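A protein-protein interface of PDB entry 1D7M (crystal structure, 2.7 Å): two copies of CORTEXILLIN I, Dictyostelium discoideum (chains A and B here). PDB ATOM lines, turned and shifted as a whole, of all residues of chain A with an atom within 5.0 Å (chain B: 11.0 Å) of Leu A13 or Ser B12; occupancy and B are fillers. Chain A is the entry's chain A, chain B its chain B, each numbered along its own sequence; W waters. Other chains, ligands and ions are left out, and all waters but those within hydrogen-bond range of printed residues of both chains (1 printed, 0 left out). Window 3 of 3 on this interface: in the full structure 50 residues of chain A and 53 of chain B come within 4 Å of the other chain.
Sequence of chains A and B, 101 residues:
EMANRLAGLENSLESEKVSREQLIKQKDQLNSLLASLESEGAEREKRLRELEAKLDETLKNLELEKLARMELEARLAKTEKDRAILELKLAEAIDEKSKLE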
ATOM      1  N   LEU A   9      -3.789  -2.528  21.924  1.00  0.00           N
ATOM      2  CA  LEU A   9      -4.711  -1.496  22.341  1.00  0.00           C
ATOM      3  C   LEU A   9      -4.021  -0.237  22.846  1.00  0.00           C
ATOM      4  O   LEU A   9      -4.595   0.846  22.778  1.00  0.00           O
ATOM      5  CB  LEU A   9      -5.697  -2.023  23.384  1.00  0.00           C
ATOM      6  CG  LEU A   9      -6.863  -2.704  22.666  1.00  0.00           C
ATOM      7  CD1 LEU A   9      -7.988  -3.035  23.649  1.00  0.00           C
ATOM      8  CD2 LEU A   9      -7.359  -1.771  21.556  1.00  0.00           C
ATOM      9  N   GLU A  10      -2.795  -0.352  23.348  1.00  0.00           N
ATOM     10  CA  GLU A  10      -2.109   0.848  23.809  1.00  0.00           C
ATOM     11  C   GLU A  10      -1.743   1.649  22.579  1.00  0.00           C
ATOM     12  O   GLU A  10      -1.669   2.873  22.621  1.00  0.00           O
ATOM     13  CB  GLU A  10      -0.830   0.517  24.563  1.00  0.00           C
ATOM     14  CG  GLU A  10      -1.018  -0.322  25.789  1.00  0.00           C
ATOM     15  CD  GLU A  10       0.299  -0.597  26.470  1.00  0.00           C
ATOM     16  OE1 GLU A  10       0.711   0.221  27.320  1.00  0.00           O
ATOM     17  OE2 GLU A  10       0.929  -1.623  26.134  1.00  0.00           O
ATOM     18  N   ASN A  11      -1.496   0.956  21.477  1.00  0.00           N
ATOM     19  CA  ASN A  11      -1.157   1.656  20.256  1.00  0.00           C
ATOM     20  C   ASN A  11      -2.387   2.423  19.773  1.00  0.00           C
ATOM     21  O   ASN A  11      -2.310   3.605  19.436  1.00  0.00           O
ATOM     22  CB  ASN A  11      -0.710   0.691  19.171  1.00  0.00           C
ATOM     23  CG  ASN A  11      -0.131   1.416  17.986  1.00  0.00           C
ATOM     24  OD1 ASN A  11       0.903   2.075  18.105  1.00  0.00           O
ATOM     25  ND2 ASN A  11      -0.801   1.325  16.837  1.00  0.00           N
ATOM     26  N   SER A  12      -3.518   1.728  19.730  1.00  0.00           N
ATOM     27  CA  SER A  12      -4.785   2.324  19.317  1.00  0.00           C
ATOM     28  C   SER A  12      -5.079   3.578  20.161  1.00  0.00           C
ATOM     29  O   SER A  12      -5.212   4.688  19.626  1.00  0.00           O
ATOM     30  CB  SER A  12      -5.908   1.286  19.467  1.00  0.00           C
ATOM     31  OG  SER A  12      -7.177   1.854  19.192  1.00  0.00           O
ATOM     32  N   LEU A  13      -5.168   3.402  21.481  1.00  0.00           N
ATOM     33  CA  LEU A  13      -5.424   4.529  22.386  1.00  0.00           C
ATOM     34  C   LEU A  13      -4.448   5.662  22.066  1.00  0.00           C
ATOM     35  O   LEU A  13      -4.806   6.835  22.074  1.00  0.00           O
ATOM     36  CB  LEU A  13      -5.241   4.114  23.854  1.00  0.00           C
ATOM     37  CG  LEU A  13      -5.695   5.201  24.840  1.00  0.00           C
ATOM     38  CD1 LEU A  13      -7.213   5.362  24.750  1.00  0.00           C
ATOM     39  CD2 LEU A  13      -5.285   4.849  26.262  1.00  0.00           C
ATOM     40  N   GLU A  14      -3.212   5.298  21.775  1.00  0.00           N
ATOM     41  CA  GLU A  14      -2.194   6.278  21.455  1.00  0.00           C
ATOM     42  C   GLU A  14      -2.555   7.203  20.291  1.00  0.00           C
ATOM     43  O   GLU A  14      -2.714   8.425  20.437  1.00  0.00           O
ATOM     44  CB  GLU A  14      -0.892   5.551  21.136  1.00  0.00           C
ATOM     45  CG  GLU A  14       0.175   6.476  20.695  1.00  0.00           C
ATOM     46  CD  GLU A  14       0.272   7.640  21.632  1.00  0.00           C
ATOM     47  OE1 GLU A  14       0.903   8.638  21.251  1.00  0.00           O
ATOM     48  OE2 GLU A  14      -0.286   7.549  22.749  1.00  0.00           O
ATOM     49  N   SER A  15      -2.675   6.609  19.116  1.00  0.00           N
ATOM     50  CA  SER A  15      -2.981   7.407  17.954  1.00  0.00           C
ATOM     51  C   SER A  15      -4.260   8.203  18.200  1.00  0.00           C
ATOM     52  O   SER A  15      -4.363   9.342  17.765  1.00  0.00           O
ATOM     53  CB  SER A  15      -3.112   6.530  16.712  1.00  0.00           C
ATOM     54  OG  SER A  15      -4.412   5.994  16.616  1.00  0.00           O
ATOM     55  N   GLU A  16      -5.224   7.628  18.915  1.00  0.00           N
ATOM     56  CA  GLU A  16      -6.467   8.345  19.183  1.00  0.00           C
ATOM     57  C   GLU A  16      -6.364   9.563  20.116  1.00  0.00           C
ATOM     58  O   GLU A  16      -7.108  10.531  19.954  1.00  0.00           O
ATOM     59  CB  GLU A  16      -7.528   7.376  19.690  1.00  0.00           C
ATOM     60  CG  GLU A  16      -8.255   6.676  18.571  1.00  0.00           C
ATOM     61  CD  GLU A  16      -9.134   5.567  19.094  1.00  0.00           C
ATOM     62  OE1 GLU A  16      -9.554   5.676  20.262  1.00  0.00           O
ATOM     63  OE2 GLU A  16      -9.409   4.599  18.352  1.00  0.00           O
ATOM     64  N   LYS A  17      -5.475   9.549  21.102  1.00  0.00           N
ATOM     65  CA  LYS A  17      -5.378  10.756  21.912  1.00  0.00           C
ATOM     66  C   LYS A  17      -4.760  11.816  21.004  1.00  0.00           C
ATOM     67  O   LYS A  17      -5.079  12.996  21.102  1.00  0.00           O
ATOM     68  CB  LYS A  17      -4.519  10.555  23.159  1.00  0.00           C
ATOM     69  CG  LYS A  17      -5.260   9.904  24.308  1.00  0.00           C
ATOM     70  CD  LYS A  17      -4.560  10.189  25.624  1.00  0.00           C
ATOM     71  CE  LYS A  17      -5.311   9.567  26.794  1.00  0.00           C
ATOM     72  NZ  LYS A  17      -4.746   9.954  28.121  1.00  0.00           N
ATOM     73  N   ASN B   4      -7.090  -7.512  33.051  1.00  0.00           N
ATOM     74  CA  ASN B   4      -7.516  -6.243  33.625  1.00  0.00           C
ATOM     75  C   ASN B   4      -7.036  -5.094  32.754  1.00  0.00           C
ATOM     76  O   ASN B   4      -7.850  -4.306  32.285  1.00  0.00           O
ATOM     77  CB  ASN B   4      -6.981  -6.059  35.045  1.00  0.00           C
ATOM     78  CG  ASN B   4      -7.850  -6.727  36.084  1.00  0.00           C
ATOM     79  OD1 ASN B   4      -7.837  -7.947  36.223  1.00  0.00           O
ATOM     80  ND2 ASN B   4      -8.622  -5.927  36.818  1.00  0.00           N
ATOM     81  N   ARG B   5      -5.726  -4.973  32.536  1.00  0.00           N
ATOM     82  CA  ARG B   5      -5.256  -3.887  31.682  1.00  0.00           C
ATOM     83  C   ARG B   5      -6.100  -3.888  30.416  1.00  0.00           C
ATOM     84  O   ARG B   5      -6.352  -2.836  29.833  1.00  0.00           O
ATOM     85  CB  ARG B   5      -3.778  -4.031  31.299  1.00  0.00           C
ATOM     86  CG  ARG B   5      -2.802  -3.392  32.271  1.00  0.00           C
ATOM     87  CD  ARG B   5      -1.461  -3.091  31.592  1.00  0.00           C
ATOM     88  NE  ARG B   5      -1.418  -1.760  30.982  1.00  0.00           N
ATOM     89  CZ  ARG B   5      -0.425  -1.315  30.214  1.00  0.00           C
ATOM     90  NH1 ARG B   5       0.613  -2.098  29.950  1.00  0.00           N
ATOM     91  NH2 ARG B   5      -0.457  -0.081  29.723  1.00  0.00           N
ATOM     92  N   LEU B   6      -6.550  -5.066  29.993  1.00  0.00           N
ATOM     93  CA  LEU B   6      -7.382  -5.152  28.794  1.00  0.00           C
ATOM     94  C   LEU B   6      -8.692  -4.358  29.021  1.00  0.00           C
ATOM     95  O   LEU B   6      -9.011  -3.447  28.256  1.00  0.00           O
ATOM     96  CB  LEU B   6      -7.669  -6.631  28.443  1.00  0.00           C
ATOM     97  CG  LEU B   6      -7.376  -7.130  27.009  1.00  0.00           C
ATOM     98  CD1 LEU B   6      -5.864  -7.095  26.743  1.00  0.00           C
ATOM     99  CD2 LEU B   6      -7.924  -8.556  26.801  1.00  0.00           C
ATOM    100  N   ALA B   7      -9.437  -4.689  30.073  1.00  0.00           N
ATOM    101  CA  ALA B   7     -10.687  -3.986  30.379  1.00  0.00           C
ATOM    102  C   ALA B   7     -10.503  -2.471  30.497  1.00  0.00           C
ATOM    103  O   ALA B   7     -11.297  -1.683  29.976  1.00  0.00           O
ATOM    104  CB  ALA B   7     -11.293  -4.524  31.673  1.00  0.00           C
ATOM    105  N   GLY B   8      -9.458  -2.059  31.199  1.00  0.00           N
ATOM    106  CA  GLY B   8      -9.228  -0.638  31.368  1.00  0.00           C
ATOM    107  C   GLY B   8      -8.862   0.064  30.082  1.00  0.00           C
ATOM    108  O   GLY B   8      -9.187   1.237  29.907  1.00  0.00           O
ATOM    109  N   LEU B   9      -8.175  -0.631  29.180  1.00  0.00           N
ATOM    110  CA  LEU B   9      -7.802   0.010  27.934  1.00  0.00           C
ATOM    111  C   LEU B   9      -9.033   0.195  27.092  1.00  0.00           C
ATOM    112  O   LEU B   9      -9.215   1.226  26.462  1.00  0.00           O
ATOM    113  CB  LEU B   9      -6.743  -0.797  27.189  1.00  0.00           C
ATOM    114  CG  LEU B   9      -5.355  -0.221  27.497  1.00  0.00           C
ATOM    115  CD1 LEU B   9      -4.302  -1.159  26.983  1.00  0.00           C
ATOM    116  CD2 LEU B   9      -5.181   1.154  26.856  1.00  0.00           C
ATOM    117  N   GLU B  10      -9.902  -0.795  27.087  1.00  0.00           N
ATOM    118  CA  GLU B  10     -11.121  -0.637  26.329  1.00  0.00           C
ATOM    119  C   GLU B  10     -11.892   0.537  26.927  1.00  0.00           C
ATOM    120  O   GLU B  10     -12.511   1.325  26.207  1.00  0.00           O
ATOM    121  CB  GLU B  10     -11.936  -1.904  26.450  1.00  0.00           C
ATOM    122  CG  GLU B  10     -11.155  -3.122  26.050  1.00  0.00           C
ATOM    123  CD  GLU B  10     -11.791  -4.366  26.582  1.00  0.00           C
ATOM    124  OE1 GLU B  10     -11.590  -4.656  27.778  1.00  0.00           O
ATOM    125  OE2 GLU B  10     -12.508  -5.037  25.812  1.00  0.00           O
ATOM    126  N   ASN B  11     -11.852   0.642  28.250  1.00  0.00           N
ATOM    127  CA  ASN B  11     -12.578   1.696  28.940  1.00  0.00           C
ATOM    128  C   ASN B  11     -12.095   3.049  28.486  1.00  0.00           C
ATOM    129  O   ASN B  11     -12.879   3.949  28.193  1.00  0.00           O
ATOM    130  CB  ASN B  11     -12.412   1.560  30.460  1.00  0.00           C
ATOM    131  CG  ASN B  11     -13.332   0.502  31.058  1.00  0.00           C
ATOM    132  OD1 ASN B  11     -14.290   0.073  30.416  1.00  0.00           O
ATOM    133  ND2 ASN B  11     -13.057   0.091  32.295  1.00  0.00           N
ATOM    134  N   SER B  12     -10.779   3.152  28.411  1.00  0.00           N
ATOM    135  CA  SER B  12     -10.091   4.365  28.022  1.00  0.00           C
ATOM    136  C   SER B  12     -10.383   4.696  26.557  1.00  0.00           C
ATOM    137  O   SER B  12     -10.479   5.863  26.164  1.00  0.00           O
ATOM    138  CB  SER B  12      -8.595   4.146  28.267  1.00  0.00           C
ATOM    139  OG  SER B  12      -7.879   5.356  28.287  1.00  0.00           O
ATOM    140  N   LEU B  13     -10.545   3.652  25.759  1.00  0.00           N
ATOM    141  CA  LEU B  13     -10.810   3.810  24.337  1.00  0.00           C
ATOM    142  C   LEU B  13     -12.215   4.371  24.125  1.00  0.00           C
ATOM    143  O   LEU B  13     -12.440   5.241  23.274  1.00  0.00           O
ATOM    144  CB  LEU B  13     -10.643   2.449  23.657  1.00  0.00           C
ATOM    145  CG  LEU B  13      -9.554   2.312  22.579  1.00  0.00           C
ATOM    146  CD1 LEU B  13      -8.311   3.116  22.948  1.00  0.00           C
ATOM    147  CD2 LEU B  13      -9.203   0.830  22.385  1.00  0.00           C
ATOM    148  N   GLU B  14     -13.147   3.874  24.922  1.00  0.00           N
ATOM    149  CA  GLU B  14     -14.533   4.303  24.862  1.00  0.00           C
ATOM    150  C   GLU B  14     -14.675   5.755  25.343  1.00  0.00           C
ATOM    151  O   GLU B  14     -15.495   6.511  24.835  1.00  0.00           O
ATOM    152  CB  GLU B  14     -15.374   3.356  25.721  1.00  0.00           C
ATOM    153  CG  GLU B  14     -16.805   3.800  25.921  1.00  0.00           C
ATOM    154  CD  GLU B  14     -17.591   3.827  24.627  1.00  0.00           C
ATOM    155  OE1 GLU B  14     -18.713   4.366  24.628  1.00  0.00           O
ATOM    156  OE2 GLU B  14     -17.092   3.303  23.616  1.00  0.00           O
ATOM    157  N   SER B  15     -13.874   6.143  26.328  1.00  0.00           N
ATOM    158  CA  SER B  15     -13.943   7.508  26.835  1.00  0.00           C
ATOM    159  C   SER B  15     -13.349   8.463  25.797  1.00  0.00           C
ATOM    160  O   SER B  15     -13.774   9.615  25.674  1.00  0.00           O
ATOM    161  CB  SER B  15     -13.193   7.620  28.160  1.00  0.00           C
ATOM    162  OG  SER B  15     -13.104   8.965  28.590  1.00  0.00           O
ATOM    163  N   GLU B  16     -12.356   7.982  25.054  1.00  0.00           N
ATOM    164  CA  GLU B  16     -11.739   8.791  24.017  1.00  0.00           C
ATOM    165  C   GLU B  16     -12.734   8.913  22.876  1.00  0.00           C
ATOM    166  O   GLU B  16     -12.785   9.933  22.200  1.00  0.00           O
ATOM    167  CB  GLU B  16     -10.440   8.149  23.522  1.00  0.00           C
ATOM    168  CG  GLU B  16      -9.238   8.401  24.430  1.00  0.00           C
ATOM    169  CD  GLU B  16      -8.758   9.850  24.386  1.00  0.00           C
ATOM    170  OE1 GLU B  16      -8.946  10.502  23.347  1.00  0.00           O
ATOM    171  OE2 GLU B  16      -8.171  10.336  25.378  1.00  0.00           O
ATOM    172  N   LYS B  17     -13.533   7.870  22.681  1.00  0.00           N
ATOM    173  CA  LYS B  17     -14.552   7.847  21.635  1.00  0.00           C
ATOM    174  C   LYS B  17     -15.600   8.933  21.929  1.00  0.00           C
ATOM    175  O   LYS B  17     -15.864   9.791  21.092  1.00  0.00           O
ATOM    176  CB  LYS B  17     -15.205   6.459  21.597  1.00  0.00           C
ATOM    177  CG  LYS B  17     -16.120   6.179  20.403  1.00  0.00           C
ATOM    178  CD  LYS B  17     -17.251   5.201  20.764  1.00  0.00           C
ATOM    179  CE  LYS B  17     -18.024   4.803  19.503  1.00  0.00           C
ATOM    180  NZ  LYS B  17     -19.242   3.949  19.684  1.00  0.00           N
ATOM    181  N   VAL B  18     -16.201   8.896  23.116  1.00  0.00           N
ATOM    182  CA  VAL B  18     -17.191   9.904  23.472  1.00  0.00           C
ATOM    183  C   VAL B  18     -16.577  11.283  23.256  1.00  0.00           C
ATOM    184  O   VAL B  18     -17.204  12.140  22.654  1.00  0.00           O
ATOM    185  CB  VAL B  18     -17.651   9.752  24.934  1.00  0.00           C
ATOM    186  CG1 VAL B  18     -18.744  10.795  25.295  1.00  0.00           C
ATOM    187  CG2 VAL B  18     -18.152   8.340  25.134  1.00  0.00           C
ATOM    188  N   SER B  19     -15.356  11.523  23.726  1.00  0.00           N
ATOM    189  CA  SER B  19     -14.744  12.838  23.496  1.00  0.00           C
ATOM    190  C   SER B  19     -14.709  13.196  21.994  1.00  0.00           C
ATOM    191  O   SER B  19     -15.195  14.251  21.553  1.00  0.00           O
ATOM    192  CB  SER B  19     -13.327  12.869  24.088  1.00  0.00           C
ATOM    193  OG  SER B  19     -13.358  12.913  25.497  1.00  0.00           O
ATOM    194  N   ARG B  20     -14.122  12.296  21.216  1.00  0.00           N
ATOM    195  CA  ARG B  20     -14.000  12.434  19.768  1.00  0.00           C
ATOM    196  C   ARG B  20     -15.331  12.820  19.093  1.00  0.00           C
ATOM    197  O   ARG B  20     -15.398  13.760  18.289  1.00  0.00           O
ATOM    198  CB  ARG B  20     -13.477  11.096  19.237  1.00  0.00           C
ATOM    199  CG  ARG B  20     -13.054  11.083  17.796  1.00  0.00           C
ATOM    200  CD  ARG B  20     -12.163   9.877  17.530  1.00  0.00           C
ATOM    201  NE  ARG B  20     -12.807   8.605  17.837  1.00  0.00           N
ATOM    202  CZ  ARG B  20     -12.280   7.651  18.603  1.00  0.00           C
ATOM    203  NH1 ARG B  20     -11.087   7.822  19.156  1.00  0.00           N
ATOM    204  NH2 ARG B  20     -12.943   6.518  18.813  1.00  0.00           N
ATOM    205  N   GLU B  21     -16.391  12.099  19.438  1.00  0.00           N
ATOM    206  CA  GLU B  21     -17.701  12.368  18.863  1.00  0.00           C
ATOM    207  C   GLU B  21     -18.177  13.764  19.267  1.00  0.00           C
ATOM    208  O   GLU B  21     -18.759  14.479  18.450  1.00  0.00           O
ATOM    209  CB  GLU B  21     -18.727  11.336  19.323  1.00  0.00           C
ATOM    210  CG  GLU B  21     -18.349   9.872  19.143  1.00  0.00           C
ATOM    211  CD  GLU B  21     -19.419   8.968  19.736  1.00  0.00           C
ATOM    212  OE1 GLU B  21     -19.948   9.346  20.799  1.00  0.00           O
ATOM    213  OE2 GLU B  21     -19.725   7.904  19.155  1.00  0.00           O
HETATM  214  O   HOH W   1     -11.872   5.296  20.763  1.00  0.00           O
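Hydrophobic or aromatic side chains of chain B that line the printed part of chain A: Leu B9 and Leu B13. Along chain B the printed residues that touch a printed residue of chain A span positions 5 to 20.
NH2 of Arg B5 lies within salt-bridge range of OE1 of Glu A10 (2.7 Å). The side-chain carboxylate (OE1) of Glu A16 is in salt-bridge range of the guanidinium group (NH1) of Arg B20.
O of Ser A12 is in hydrogen-bond range of OG of Ser A15 (3.4 Å). N of Ala B7 sits close to OE1 of Glu B10, 3.1 Å away.
Water W1 lies within hydrogen-bond range of OE1 of Glu A16, NH2 of Arg B20 and O of Leu B13.
Among the printed residues, merely in contact across the chains: Leu A13 with Leu B13, Lys A17 with Glu B16, Leu A9 with Leu B13, Leu A13 with Ser B12, Glu A10 with Leu B9, Leu A13 with Glu B16, Leu A13 with Leu B9, Glu A16 with Glu B16, Glu A16 with Leu B13, Ser A12 with Leu B13, Leu A9 with Leu B9 and Leu A9 with Glu B10.
Leu A9 touches its own counterpart, Leu B9. Leu A9 touches Leu B13, and with the chains exchanged Leu A13 touches Leu B9. Leu A13 touches Glu B16, and with the chains exchanged Glu A16 touches Leu B13. Lys A17 touches Glu B16, but with the chains exchanged Glu A16 does not touch Lys B17 (5.1 Å). Of the 14 pairs that touch across the chains among the printed residues, 11 have their exchanged pair printed and touching as well.
Leu A13 touches just these residues of chain B: Leu B9 (3.7 Å), Ser B12 (3.3 Å), Leu B13 (3.1 Å) and Glu B16 (3.7 Å). Of chain B, only Leu B13 (3.9 Å) comes within 4 Å of Ser A12. No residue of chain B comes within 4 Å of Glu A14. Glu A16 touches just these residues of chain B: Leu B13 (3.9 Å), Glu B16 (3.9 Å) and Arg B20 (2.9 Å). Lys A17 touches one residue of chain B. Printed residues of chain B within 4 Å of Glu A10: Arg B5 and Leu B9. Printed residues of chain A within 4 Å of Arg B5: Glu A10. Asn B11 touches none of the printed residues of chain A. Leu B6 touches none of the printed residues of chain A. The nearest printed residue of chain A that does not touch Arg B5 is Leu A9 (6.4 Å).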
